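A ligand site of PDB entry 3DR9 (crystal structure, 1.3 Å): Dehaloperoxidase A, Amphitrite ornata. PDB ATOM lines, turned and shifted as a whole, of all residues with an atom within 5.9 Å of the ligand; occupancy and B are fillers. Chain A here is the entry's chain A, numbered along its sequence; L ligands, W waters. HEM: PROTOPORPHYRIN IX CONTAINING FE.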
ATOM      1  N   PHE A  24     -13.980  -5.302  -9.428  1.00  0.00           N
ATOM      2  CA  PHE A  24     -14.230  -5.707  -8.056  1.00  0.00           C
ATOM      3  C   PHE A  24     -13.035  -6.441  -7.450  1.00  0.00           C
ATOM      4  O   PHE A  24     -12.534  -6.042  -6.377  1.00  0.00           O
ATOM      5  CB  PHE A  24     -15.505  -6.556  -8.027  1.00  0.00           C
ATOM      6  CG  PHE A  24     -15.719  -7.331  -6.755  1.00  0.00           C
ATOM      7  CD1 PHE A  24     -15.872  -6.686  -5.521  1.00  0.00           C
ATOM      8  CD2 PHE A  24     -15.844  -8.709  -6.796  1.00  0.00           C
ATOM      9  CE1 PHE A  24     -16.121  -7.413  -4.361  1.00  0.00           C
ATOM     10  CE2 PHE A  24     -16.074  -9.451  -5.629  1.00  0.00           C
ATOM     11  CZ  PHE A  24     -16.219  -8.794  -4.421  1.00  0.00           C
ATOM     12  N   GLU A  31     -10.912 -10.575  -2.000  1.00  0.00           N
ATOM     13  CA  GLU A  31     -12.180 -11.215  -2.367  1.00  0.00           C
ATOM     14  C   GLU A  31     -11.980 -12.380  -3.330  1.00  0.00           C
ATOM     15  O   GLU A  31     -12.868 -13.231  -3.479  1.00  0.00           O
ATOM     16  CB  GLU A  31     -13.168 -10.198  -2.946  1.00  0.00           C
ATOM     17  CG  GLU A  31     -13.528  -9.052  -2.010  1.00  0.00           C
ATOM     18  CD  GLU A  31     -14.313  -9.511  -0.797  1.00  0.00           C
ATOM     19  OE1 GLU A  31     -15.491  -9.896  -0.942  1.00  0.00           O
ATOM     20  OE2 GLU A  31     -13.758  -9.470   0.318  1.00  0.00           O
ATOM     21  N   TYR A  34     -12.669 -16.287  -2.542  1.00  0.00           N
ATOM     22  CA  TYR A  34     -13.972 -16.950  -2.647  1.00  0.00           C
ATOM     23  C   TYR A  34     -14.124 -17.701  -3.974  1.00  0.00           C
ATOM     24  O   TYR A  34     -15.054 -18.482  -4.149  1.00  0.00           O
ATOM     25  CB  TYR A  34     -15.101 -15.929  -2.495  1.00  0.00           C
ATOM     26  CG  TYR A  34     -15.193 -15.272  -1.124  1.00  0.00           C
ATOM     27  CD1 TYR A  34     -15.751 -15.960  -0.043  1.00  0.00           C
ATOM     28  CD2 TYR A  34     -14.745 -13.967  -0.907  1.00  0.00           C
ATOM     29  CE1 TYR A  34     -15.838 -15.357   1.216  1.00  0.00           C
ATOM     30  CE2 TYR A  34     -14.820 -13.371   0.349  1.00  0.00           C
ATOM     31  CZ  TYR A  34     -15.379 -14.060   1.398  1.00  0.00           C
ATOM     32  OH  TYR A  34     -15.460 -13.467   2.635  1.00  0.00           O
ATOM     33  N   PHE A  35     -13.208 -17.433  -4.906  1.00  0.00           N
ATOM     34  CA  PHE A  35     -13.271 -17.999  -6.236  1.00  0.00           C
ATOM     35  C   PHE A  35     -11.966 -18.749  -6.445  1.00  0.00           C
ATOM     36  O   PHE A  35     -11.047 -18.251  -7.112  1.00  0.00           O
ATOM     37  CB  PHE A  35     -13.427 -16.879  -7.257  1.00  0.00           C
ATOM     38  CG  PHE A  35     -14.646 -16.030  -7.038  1.00  0.00           C
ATOM     39  CD1 PHE A  35     -14.596 -14.899  -6.232  1.00  0.00           C
ATOM     40  CD2 PHE A  35     -15.849 -16.376  -7.618  1.00  0.00           C
ATOM     41  CE1 PHE A  35     -15.744 -14.123  -6.027  1.00  0.00           C
ATOM     42  CE2 PHE A  35     -16.994 -15.609  -7.413  1.00  0.00           C
ATOM     43  CZ  PHE A  35     -16.945 -14.489  -6.616  1.00  0.00           C
ATOM     44  N   TYR A  38      -9.803 -19.016  -9.691  1.00  0.00           N
ATOM     45  CA  TYR A  38      -9.317 -17.813 -10.370  1.00  0.00           C
ATOM     46  C   TYR A  38      -8.035 -17.254  -9.741  1.00  0.00           C
ATOM     47  O   TYR A  38      -7.460 -16.291 -10.258  1.00  0.00           O
ATOM     48  CB  TYR A  38     -10.424 -16.753 -10.476  1.00  0.00           C
ATOM     49  CG  TYR A  38     -11.754 -17.282 -11.008  1.00  0.00           C
ATOM     50  CD1 TYR A  38     -11.817 -18.387 -11.856  1.00  0.00           C
ATOM     51  CD2 TYR A  38     -12.958 -16.665 -10.665  1.00  0.00           C
ATOM     52  CE1 TYR A  38     -13.040 -18.871 -12.335  1.00  0.00           C
ATOM     53  CE2 TYR A  38     -14.184 -17.139 -11.144  1.00  0.00           C
ATOM     54  CZ  TYR A  38     -14.216 -18.244 -11.971  1.00  0.00           C
ATOM     55  OH  TYR A  38     -15.418 -18.711 -12.438  1.00  0.00           O
ATOM     56  N   LYS A  51     -15.867 -21.519 -17.420  1.00  0.00           N
ATOM     57  CA  LYS A  51     -16.717 -21.185 -16.296  1.00  0.00           C
ATOM     58  C   LYS A  51     -16.514 -19.747 -15.810  1.00  0.00           C
ATOM     59  O   LYS A  51     -17.426 -19.178 -15.210  1.00  0.00           O
ATOM     60  CB  LYS A  51     -16.571 -22.168 -15.141  1.00  0.00           C
ATOM     61  CG  LYS A  51     -17.073 -23.567 -15.453  1.00  0.00           C
ATOM     62  CD  LYS A  51     -17.047 -24.426 -14.199  1.00  0.00           C
ATOM     63  CE  LYS A  51     -17.770 -25.743 -14.446  1.00  0.00           C
ATOM     64  NZ  LYS A  51     -17.609 -26.701 -13.321  1.00  0.00           N
ATOM     65  N   ASP A  54     -18.896 -17.866 -18.151  1.00  0.00           N
ATOM     66  CA  ASP A  54     -20.250 -18.390 -18.023  1.00  0.00           C
ATOM     67  C   ASP A  54     -20.850 -18.014 -16.682  1.00  0.00           C
ATOM     68  O   ASP A  54     -21.967 -17.474 -16.604  1.00  0.00           O
ATOM     69  CB  ASP A  54     -20.235 -19.918 -18.188  1.00  0.00           C
ATOM     70  CG  ASP A  54     -21.632 -20.522 -18.173  1.00  0.00           C
ATOM     71  OD1 ASP A  54     -22.276 -20.588 -19.253  1.00  0.00           O
ATOM     72  OD2 ASP A  54     -22.072 -20.964 -17.092  1.00  0.00           O
ATOM     73  N   HIS A  55     -20.101 -18.304 -15.631  1.00  0.00           N
ATOM     74  CA  HIS A  55     -20.594 -18.094 -14.282  1.00  0.00           C
ATOM     75  C   HIS A  55     -20.658 -16.606 -13.956  1.00  0.00           C
ATOM     76  O   HIS A  55     -21.593 -16.158 -13.309  1.00  0.00           O
ATOM     77  CB  HIS A  55     -19.725 -18.862 -13.280  1.00  0.00           C
ATOM     78  CG  HIS A  55     -19.900 -20.350 -13.331  1.00  0.00           C
ATOM     79  ND1 HIS A  55     -19.582 -21.168 -12.269  1.00  0.00           N
ATOM     80  CD2 HIS A  55     -20.361 -21.173 -14.305  1.00  0.00           C
ATOM     81  CE1 HIS A  55     -19.848 -22.432 -12.586  1.00  0.00           C
ATOM     82  NE2 HIS A  55     -20.312 -22.449 -13.822  1.00  0.00           N
ATOM     83  N   THR A  56     -19.664 -15.837 -14.399  1.00  0.00           N
ATOM     84  CA  THR A  56     -19.663 -14.406 -14.152  1.00  0.00           C
ATOM     85  C   THR A  56     -20.858 -13.728 -14.857  1.00  0.00           C
ATOM     86  O   THR A  56     -21.538 -12.880 -14.280  1.00  0.00           O
ATOM     87  CB  THR A  56     -18.315 -13.767 -14.550  1.00  0.00           C
ATOM     88  OG1 THR A  56     -17.269 -14.384 -13.780  1.00  0.00           O
ATOM     89  CG2 THR A  56     -18.324 -12.265 -14.277  1.00  0.00           C
ATOM     90  N   LYS A  58     -23.677 -15.228 -15.514  1.00  0.00           N
ATOM     91  CA  LYS A  58     -24.824 -15.634 -14.706  1.00  0.00           C
ATOM     92  C   LYS A  58     -25.026 -14.794 -13.451  1.00  0.00           C
ATOM     93  O   LYS A  58     -26.154 -14.447 -13.118  1.00  0.00           O
ATOM     94  CB  LYS A  58     -24.777 -17.137 -14.426  1.00  0.00           C
ATOM     95  CG  LYS A  58     -25.108 -17.920 -15.696  1.00  0.00           C
ATOM     96  CD  LYS A  58     -24.771 -19.406 -15.658  1.00  0.00           C
ATOM     97  CE  LYS A  58     -25.127 -20.073 -16.989  1.00  0.00           C
ATOM     98  NZ  LYS A  58     -24.688 -21.487 -17.007  1.00  0.00           N
ATOM     99  N   VAL A  59     -23.923 -14.434 -12.774  1.00  0.00           N
ATOM    100  CA  VAL A  59     -24.012 -13.513 -11.655  1.00  0.00           C
ATOM    101  C   VAL A  59     -24.696 -12.220 -12.100  1.00  0.00           C
ATOM    102  O   VAL A  59     -25.644 -11.756 -11.473  1.00  0.00           O
ATOM    103  CB  VAL A  59     -22.602 -13.221 -11.096  1.00  0.00           C
ATOM    104  CG1 VAL A  59     -22.655 -12.082 -10.063  1.00  0.00           C
ATOM    105  CG2 VAL A  59     -21.999 -14.491 -10.498  1.00  0.00           C
ATOM    106  N   PHE A  60     -24.205 -11.626 -13.166  1.00  0.00           N
ATOM    107  CA  PHE A  60     -24.705 -10.329 -13.591  1.00  0.00           C
ATOM    108  C   PHE A  60     -26.069 -10.401 -14.239  1.00  0.00           C
ATOM    109  O   PHE A  60     -26.838  -9.440 -14.149  1.00  0.00           O
ATOM    110  CB  PHE A  60     -23.682  -9.585 -14.435  1.00  0.00           C
ATOM    111  CG  PHE A  60     -22.588  -8.982 -13.598  1.00  0.00           C
ATOM    112  CD1 PHE A  60     -22.622  -7.632 -13.273  1.00  0.00           C
ATOM    113  CD2 PHE A  60     -21.564  -9.771 -13.074  1.00  0.00           C
ATOM    114  CE1 PHE A  60     -21.638  -7.064 -12.488  1.00  0.00           C
ATOM    115  CE2 PHE A  60     -20.562  -9.218 -12.282  1.00  0.00           C
ATOM    116  CZ  PHE A  60     -20.615  -7.864 -11.973  1.00  0.00           C
ATOM    117  N   LEU A  62     -28.447 -12.406 -13.109  1.00  0.00           N
ATOM    118  CA  LEU A  62     -29.302 -12.323 -11.927  1.00  0.00           C
ATOM    119  C   LEU A  62     -29.339 -10.902 -11.355  1.00  0.00           C
ATOM    120  O   LEU A  62     -30.407 -10.410 -10.989  1.00  0.00           O
ATOM    121  CB  LEU A  62     -28.963 -13.376 -10.872  1.00  0.00           C
ATOM    122  CG  LEU A  62     -29.887 -13.417  -9.647  1.00  0.00           C
ATOM    123  CD1 LEU A  62     -31.375 -13.600  -9.980  1.00  0.00           C
ATOM    124  CD2 LEU A  62     -29.436 -14.512  -8.679  1.00  0.00           C
ATOM    125  N   MET A  63     -28.184 -10.235 -11.316  1.00  0.00           N
ATOM    126  CA  MET A  63     -28.166  -8.862 -10.810  1.00  0.00           C
ATOM    127  C   MET A  63     -29.116  -7.977 -11.619  1.00  0.00           C
ATOM    128  O   MET A  63     -29.848  -7.177 -11.071  1.00  0.00           O
ATOM    129  CB  MET A  63     -26.751  -8.285 -10.828  1.00  0.00           C
ATOM    130  CG  MET A  63     -26.692  -6.935 -10.120  1.00  0.00           C
ATOM    131  SD  MET A  63     -25.170  -6.018 -10.350  1.00  0.00           S
ATOM    132  CE  MET A  63     -23.990  -7.028  -9.444  1.00  0.00           C
ATOM    133  N   VAL A  66     -32.763  -8.716 -10.771  1.00  0.00           N
ATOM    134  CA  VAL A  66     -33.124  -8.102  -9.493  1.00  0.00           C
ATOM    135  C   VAL A  66     -33.283  -6.577  -9.673  1.00  0.00           C
ATOM    136  O   VAL A  66     -34.254  -5.988  -9.183  1.00  0.00           O
ATOM    137  CB  VAL A  66     -32.100  -8.453  -8.411  1.00  0.00           C
ATOM    138  CG1 VAL A  66     -32.393  -7.693  -7.134  1.00  0.00           C
ATOM    139  CG2 VAL A  66     -32.117  -9.956  -8.151  1.00  0.00           C
ATOM    140  N   LEU A  83     -30.881 -14.555  -2.873  1.00  0.00           N
ATOM    141  CA  LEU A  83     -29.442 -14.310  -2.735  1.00  0.00           C
ATOM    142  C   LEU A  83     -28.864 -14.820  -1.401  1.00  0.00           C
ATOM    143  O   LEU A  83     -27.747 -15.356  -1.362  1.00  0.00           O
ATOM    144  CB  LEU A  83     -29.155 -12.826  -2.915  1.00  0.00           C
ATOM    145  CG  LEU A  83     -29.401 -12.323  -4.342  1.00  0.00           C
ATOM    146  CD1 LEU A  83     -29.295 -10.817  -4.398  1.00  0.00           C
ATOM    147  CD2 LEU A  83     -28.455 -12.999  -5.334  1.00  0.00           C
ATOM    148  N   MET A  86     -28.807 -18.923  -1.389  1.00  0.00           N
ATOM    149  CA  MET A  86     -27.908 -19.643  -2.306  1.00  0.00           C
ATOM    150  C   MET A  86     -26.742 -20.276  -1.554  1.00  0.00           C
ATOM    151  O   MET A  86     -26.070 -19.605  -0.782  1.00  0.00           O
ATOM    152  CB  MET A  86     -27.368 -18.699  -3.384  1.00  0.00           C
ATOM    153  CG  MET A  86     -28.394 -18.348  -4.444  1.00  0.00           C
ATOM    154  SD  MET A  86     -27.812 -17.047  -5.544  1.00  0.00           S
ATOM    155  CE  MET A  86     -26.246 -17.739  -6.098  1.00  0.00           C
ATOM    156  N   GLN A  88     -23.925 -21.041  -2.576  1.00  0.00           N
ATOM    157  CA  GLN A  88     -22.672 -20.380  -2.976  1.00  0.00           C
ATOM    158  C   GLN A  88     -22.403 -19.140  -2.154  1.00  0.00           C
ATOM    159  O   GLN A  88     -21.281 -18.619  -2.136  1.00  0.00           O
ATOM    160  CB  GLN A  88     -22.688 -20.007  -4.453  1.00  0.00           C
ATOM    161  CG  GLN A  88     -23.064 -21.136  -5.382  1.00  0.00           C
ATOM    162  CD  GLN A  88     -24.506 -21.079  -5.818  1.00  0.00           C
ATOM    163  OE1 GLN A  88     -25.433 -21.010  -5.003  1.00  0.00           O
ATOM    164  NE2 GLN A  88     -24.707 -21.101  -7.122  1.00  0.00           N
ATOM    165  N   HIS A  89     -23.428 -18.645  -1.472  1.00  0.00           N
ATOM    166  CA  HIS A  89     -23.332 -17.437  -0.661  1.00  0.00           C
ATOM    167  C   HIS A  89     -23.359 -17.696   0.848  1.00  0.00           C
ATOM    168  O   HIS A  89     -23.502 -16.751   1.620  1.00  0.00           O
ATOM    169  CB  HIS A  89     -24.482 -16.502  -1.001  1.00  0.00           C
ATOM    170  CG  HIS A  89     -24.421 -15.924  -2.385  1.00  0.00           C
ATOM    171  ND1 HIS A  89     -25.508 -15.314  -2.979  1.00  0.00           N
ATOM    172  CD2 HIS A  89     -23.420 -15.891  -3.303  1.00  0.00           C
ATOM    173  CE1 HIS A  89     -25.164 -14.895  -4.182  1.00  0.00           C
ATOM    174  NE2 HIS A  89     -23.906 -15.230  -4.402  1.00  0.00           N
ATOM    175  N   LEU A  92     -20.866 -15.732   3.017  1.00  0.00           N
ATOM    176  CA  LEU A  92     -20.772 -14.299   2.761  1.00  0.00           C
ATOM    177  C   LEU A  92     -21.473 -13.451   3.826  1.00  0.00           C
ATOM    178  O   LEU A  92     -22.323 -13.926   4.572  1.00  0.00           O
ATOM    179  CB  LEU A  92     -21.293 -13.963   1.358  1.00  0.00           C
ATOM    180  CG  LEU A  92     -20.623 -14.708   0.204  1.00  0.00           C
ATOM    181  CD1 LEU A  92     -21.244 -14.252  -1.107  1.00  0.00           C
ATOM    182  CD2 LEU A  92     -19.110 -14.487   0.202  1.00  0.00           C
ATOM    183  N   ASN A  96     -19.506  -8.090   1.727  1.00  0.00           N
ATOM    184  CA  ASN A  96     -19.048  -8.602   0.433  1.00  0.00           C
ATOM    185  C   ASN A  96     -19.833  -7.938  -0.690  1.00  0.00           C
ATOM    186  O   ASN A  96     -19.274  -7.520  -1.712  1.00  0.00           O
ATOM    187  CB  ASN A  96     -19.193 -10.124   0.345  1.00  0.00           C
ATOM    188  CG  ASN A  96     -18.336 -10.874   1.359  1.00  0.00           C
ATOM    189  OD1 ASN A  96     -18.864 -11.495   2.281  1.00  0.00           O
ATOM    190  ND2 ASN A  96     -17.025 -10.835   1.186  1.00  0.00           N
ATOM    191  N   PHE A  97     -21.152  -7.853  -0.500  1.00  0.00           N
ATOM    192  CA  PHE A  97     -22.036  -7.193  -1.449  1.00  0.00           C
ATOM    193  C   PHE A  97     -21.795  -5.700  -1.540  1.00  0.00           C
ATOM    194  O   PHE A  97     -21.783  -5.170  -2.655  1.00  0.00           O
ATOM    195  CB  PHE A  97     -23.505  -7.527  -1.159  1.00  0.00           C
ATOM    196  CG  PHE A  97     -23.837  -8.954  -1.398  1.00  0.00           C
ATOM    197  CD1 PHE A  97     -24.499  -9.343  -2.566  1.00  0.00           C
ATOM    198  CD2 PHE A  97     -23.470  -9.941  -0.480  1.00  0.00           C
ATOM    199  CE1 PHE A  97     -24.803 -10.668  -2.798  1.00  0.00           C
ATOM    200  CE2 PHE A  97     -23.750 -11.290  -0.727  1.00  0.00           C
ATOM    201  CZ  PHE A  97     -24.422 -11.650  -1.895  1.00  0.00           C
ATOM    202  N   LEU A 100     -18.761  -5.152  -3.707  1.00  0.00           N
ATOM    203  CA  LEU A 100     -19.105  -5.326  -5.123  1.00  0.00           C
ATOM    204  C   LEU A 100     -19.750  -4.068  -5.695  1.00  0.00           C
ATOM    205  O   LEU A 100     -19.372  -3.603  -6.777  1.00  0.00           O
ATOM    206  CB  LEU A 100     -20.007  -6.550  -5.331  1.00  0.00           C
ATOM    207  CG  LEU A 100     -20.505  -6.783  -6.759  1.00  0.00           C
ATOM    208  CD1 LEU A 100     -19.368  -6.993  -7.766  1.00  0.00           C
ATOM    209  CD2 LEU A 100     -21.426  -7.984  -6.741  1.00  0.00           C
ATOM    210  N   PHE A 101     -20.679  -3.479  -4.952  1.00  0.00           N
ATOM    211  CA  PHE A 101     -21.371  -2.294  -5.444  1.00  0.00           C
ATOM    212  C   PHE A 101     -20.506  -1.036  -5.420  1.00  0.00           C
ATOM    213  O   PHE A 101     -20.629  -0.194  -6.307  1.00  0.00           O
ATOM    214  CB  PHE A 101     -22.737  -2.123  -4.769  1.00  0.00           C
ATOM    215  CG  PHE A 101     -23.769  -3.034  -5.361  1.00  0.00           C
ATOM    216  CD1 PHE A 101     -24.028  -4.265  -4.778  1.00  0.00           C
ATOM    217  CD2 PHE A 101     -24.406  -2.704  -6.553  1.00  0.00           C
ATOM    218  CE1 PHE A 101     -24.935  -5.136  -5.334  1.00  0.00           C
ATOM    219  CE2 PHE A 101     -25.319  -3.578  -7.127  1.00  0.00           C
ATOM    220  CZ  PHE A 101     -25.587  -4.790  -6.522  1.00  0.00           C
ATOM    221  N   LEU A 127     -30.153  -3.016  -1.404  1.00  0.00           N
ATOM    222  CA  LEU A 127     -29.965  -4.456  -1.459  1.00  0.00           C
ATOM    223  C   LEU A 127     -29.286  -4.979  -0.191  1.00  0.00           C
ATOM    224  O   LEU A 127     -29.722  -5.993   0.359  1.00  0.00           O
ATOM    225  CB  LEU A 127     -29.195  -4.881  -2.714  1.00  0.00           C
ATOM    226  CG  LEU A 127     -29.071  -6.398  -2.907  1.00  0.00           C
ATOM    227  CD1 LEU A 127     -30.426  -7.107  -2.977  1.00  0.00           C
ATOM    228  CD2 LEU A 127     -28.257  -6.726  -4.148  1.00  0.00           C
HETATM  229  CHA HEM L   1     -22.338 -17.770  -7.623  1.00  0.00           C
HETATM  230  CHB HEM L   1     -25.493 -14.149  -8.188  1.00  0.00           C
HETATM  231  CHC HEM L   1     -22.787 -11.352  -5.303  1.00  0.00           C
HETATM  232  CHD HEM L   1     -19.771 -15.038  -4.488  1.00  0.00           C
HETATM  233  C1A HEM L   1     -23.399 -17.032  -8.084  1.00  0.00           C
HETATM  234  C2A HEM L   1     -24.363 -17.434  -9.092  1.00  0.00           C
HETATM  235  C3A HEM L   1     -25.233 -16.429  -9.261  1.00  0.00           C
HETATM  236  C4A HEM L   1     -24.859 -15.363  -8.356  1.00  0.00           C
HETATM  237  CMA HEM L   1     -26.439 -16.412 -10.233  1.00  0.00           C
HETATM  238  CAA HEM L   1     -24.329 -18.799  -9.830  1.00  0.00           C
HETATM  239  CBA HEM L   1     -23.248 -18.799 -10.911  1.00  0.00           C
HETATM  240  CGA HEM L   1     -23.144 -20.130 -11.614  1.00  0.00           C
HETATM  241  O1A HEM L   1     -23.256 -20.144 -12.855  1.00  0.00           O
HETATM  242  O2A HEM L   1     -22.908 -21.176 -10.962  1.00  0.00           O
HETATM  243  C1B HEM L   1     -25.032 -13.064  -7.476  1.00  0.00           C
HETATM  244  C2B HEM L   1     -25.603 -11.732  -7.486  1.00  0.00           C
HETATM  245  C3B HEM L   1     -24.848 -10.961  -6.682  1.00  0.00           C
HETATM  246  C4B HEM L   1     -23.789 -11.781  -6.144  1.00  0.00           C
HETATM  247  CMB HEM L   1     -26.846 -11.344  -8.304  1.00  0.00           C
HETATM  248  CAB HEM L   1     -25.053  -9.465  -6.372  1.00  0.00           C
HETATM  249  CBB HEM L   1     -26.255  -8.877  -6.304  1.00  0.00           C
HETATM  250  C1C HEM L   1     -21.716 -12.087  -4.846  1.00  0.00           C
HETATM  251  C2C HEM L   1     -20.617 -11.598  -4.026  1.00  0.00           C
HETATM  252  C3C HEM L   1     -19.795 -12.627  -3.826  1.00  0.00           C
HETATM  253  C4C HEM L   1     -20.333 -13.786  -4.480  1.00  0.00           C
HETATM  254  CMC HEM L   1     -20.499 -10.153  -3.522  1.00  0.00           C
HETATM  255  CAC HEM L   1     -18.473 -12.676  -3.007  1.00  0.00           C
HETATM  256  CBC HEM L   1     -17.633 -11.653  -2.909  1.00  0.00           C
HETATM  257  C1D HEM L   1     -20.164 -16.085  -5.284  1.00  0.00           C
HETATM  258  C2D HEM L   1     -19.412 -17.314  -5.415  1.00  0.00           C
HETATM  259  C3D HEM L   1     -20.207 -18.165  -6.386  1.00  0.00           C
HETATM  260  C4D HEM L   1     -21.365 -17.380  -6.745  1.00  0.00           C
HETATM  261  CMD HEM L   1     -18.090 -17.693  -4.732  1.00  0.00           C
HETATM  262  CAD HEM L   1     -19.819 -19.560  -6.891  1.00  0.00           C
HETATM  263  CBD HEM L   1     -18.864 -19.330  -8.067  1.00  0.00           C
HETATM  264  CGD HEM L   1     -18.974 -20.384  -9.141  1.00  0.00           C
HETATM  265  O1D HEM L   1     -18.518 -20.064 -10.274  1.00  0.00           O
HETATM  266  O2D HEM L   1     -19.487 -21.505  -8.901  1.00  0.00           O
HETATM  267  NA  HEM L   1     -23.731 -15.759  -7.667  1.00  0.00           N
HETATM  268  NB  HEM L   1     -23.924 -13.064  -6.654  1.00  0.00           N
HETATM  269  NC  HEM L   1     -21.502 -13.432  -5.105  1.00  0.00           N
HETATM  270  ND  HEM L   1     -21.314 -16.159  -6.069  1.00  0.00           N
HETATM  271 FE   HEM L   1     -22.745 -14.695  -6.162  1.00  0.00          FE
HETATM  272  O   HOH W   1     -16.727 -19.306  -1.978  1.00  0.00           O
HETATM  273  O   HOH W   2     -28.719 -19.037 -10.033  1.00  0.00           O
HETATM  274  O   HOH W   3     -17.548 -17.609 -11.084  1.00  0.00           O
HETATM  275  O   HOH W   4     -23.805 -22.535 -13.920  1.00  0.00           O
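A ring nitrogen (ND1) of His 55 is in hydrogen-bond range of an oxygen (O1D) of the ligand, 2.5 Å away. NE2 of His 89 binds FE of the ligand.
ND2 of Asn 96 lies within hydrogen-bond range of OH of Tyr 34 (3.4 Å). ND1 of His 89 lies within hydrogen-bond range of O of Leu 83, 2.8 Å away. The side-chain amide nitrogen (ND2) of Asn 96 sits at hydrogen-bond distance from the side-chain carboxylate (OE1) of Glu 31 (2.8 Å). NZ of Lys 58 is in salt-bridge range of OD2 of Asp 54 (2.7 Å).
Merely in contact with the ligand: Phe 24, Glu 31, Tyr 34, Phe 35, Lys 58, Val 59, Leu 62, Met 63, Leu 83, Met 86, Gln 88, Leu 92, Asn 96, Phe 97, Leu 100 and Leu 127. Hydrophobic or aromatic side chains that line the ligand: Phe 24, Phe 35, His 55, Val 59, Leu 62, Met 63, Leu 83, Met 86, His 89, Leu 92, Phe 97, Leu 100 and Leu 127. Within 4 Å of the ligand: Phe 24, Glu 31, Tyr 34, Phe 35, His 55, Lys 58, Val 59, Leu 62, Met 63, Leu 83, Met 86, Gln 88, His 89, Leu 92, Asn 96, Phe 97, Leu 100 and Leu 127.
Water W4 lies within hydrogen-bond range of an oxygen (O1A) of the ligand, the side-chain amino group of Lys 58 and a ring nitrogen (NE2) of His 55. Water W3 bridges the side-chain hydroxyl (OH) of Tyr 38 (2.8 Å) and an oxygen (O1D) of the ligand (2.8 Å).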
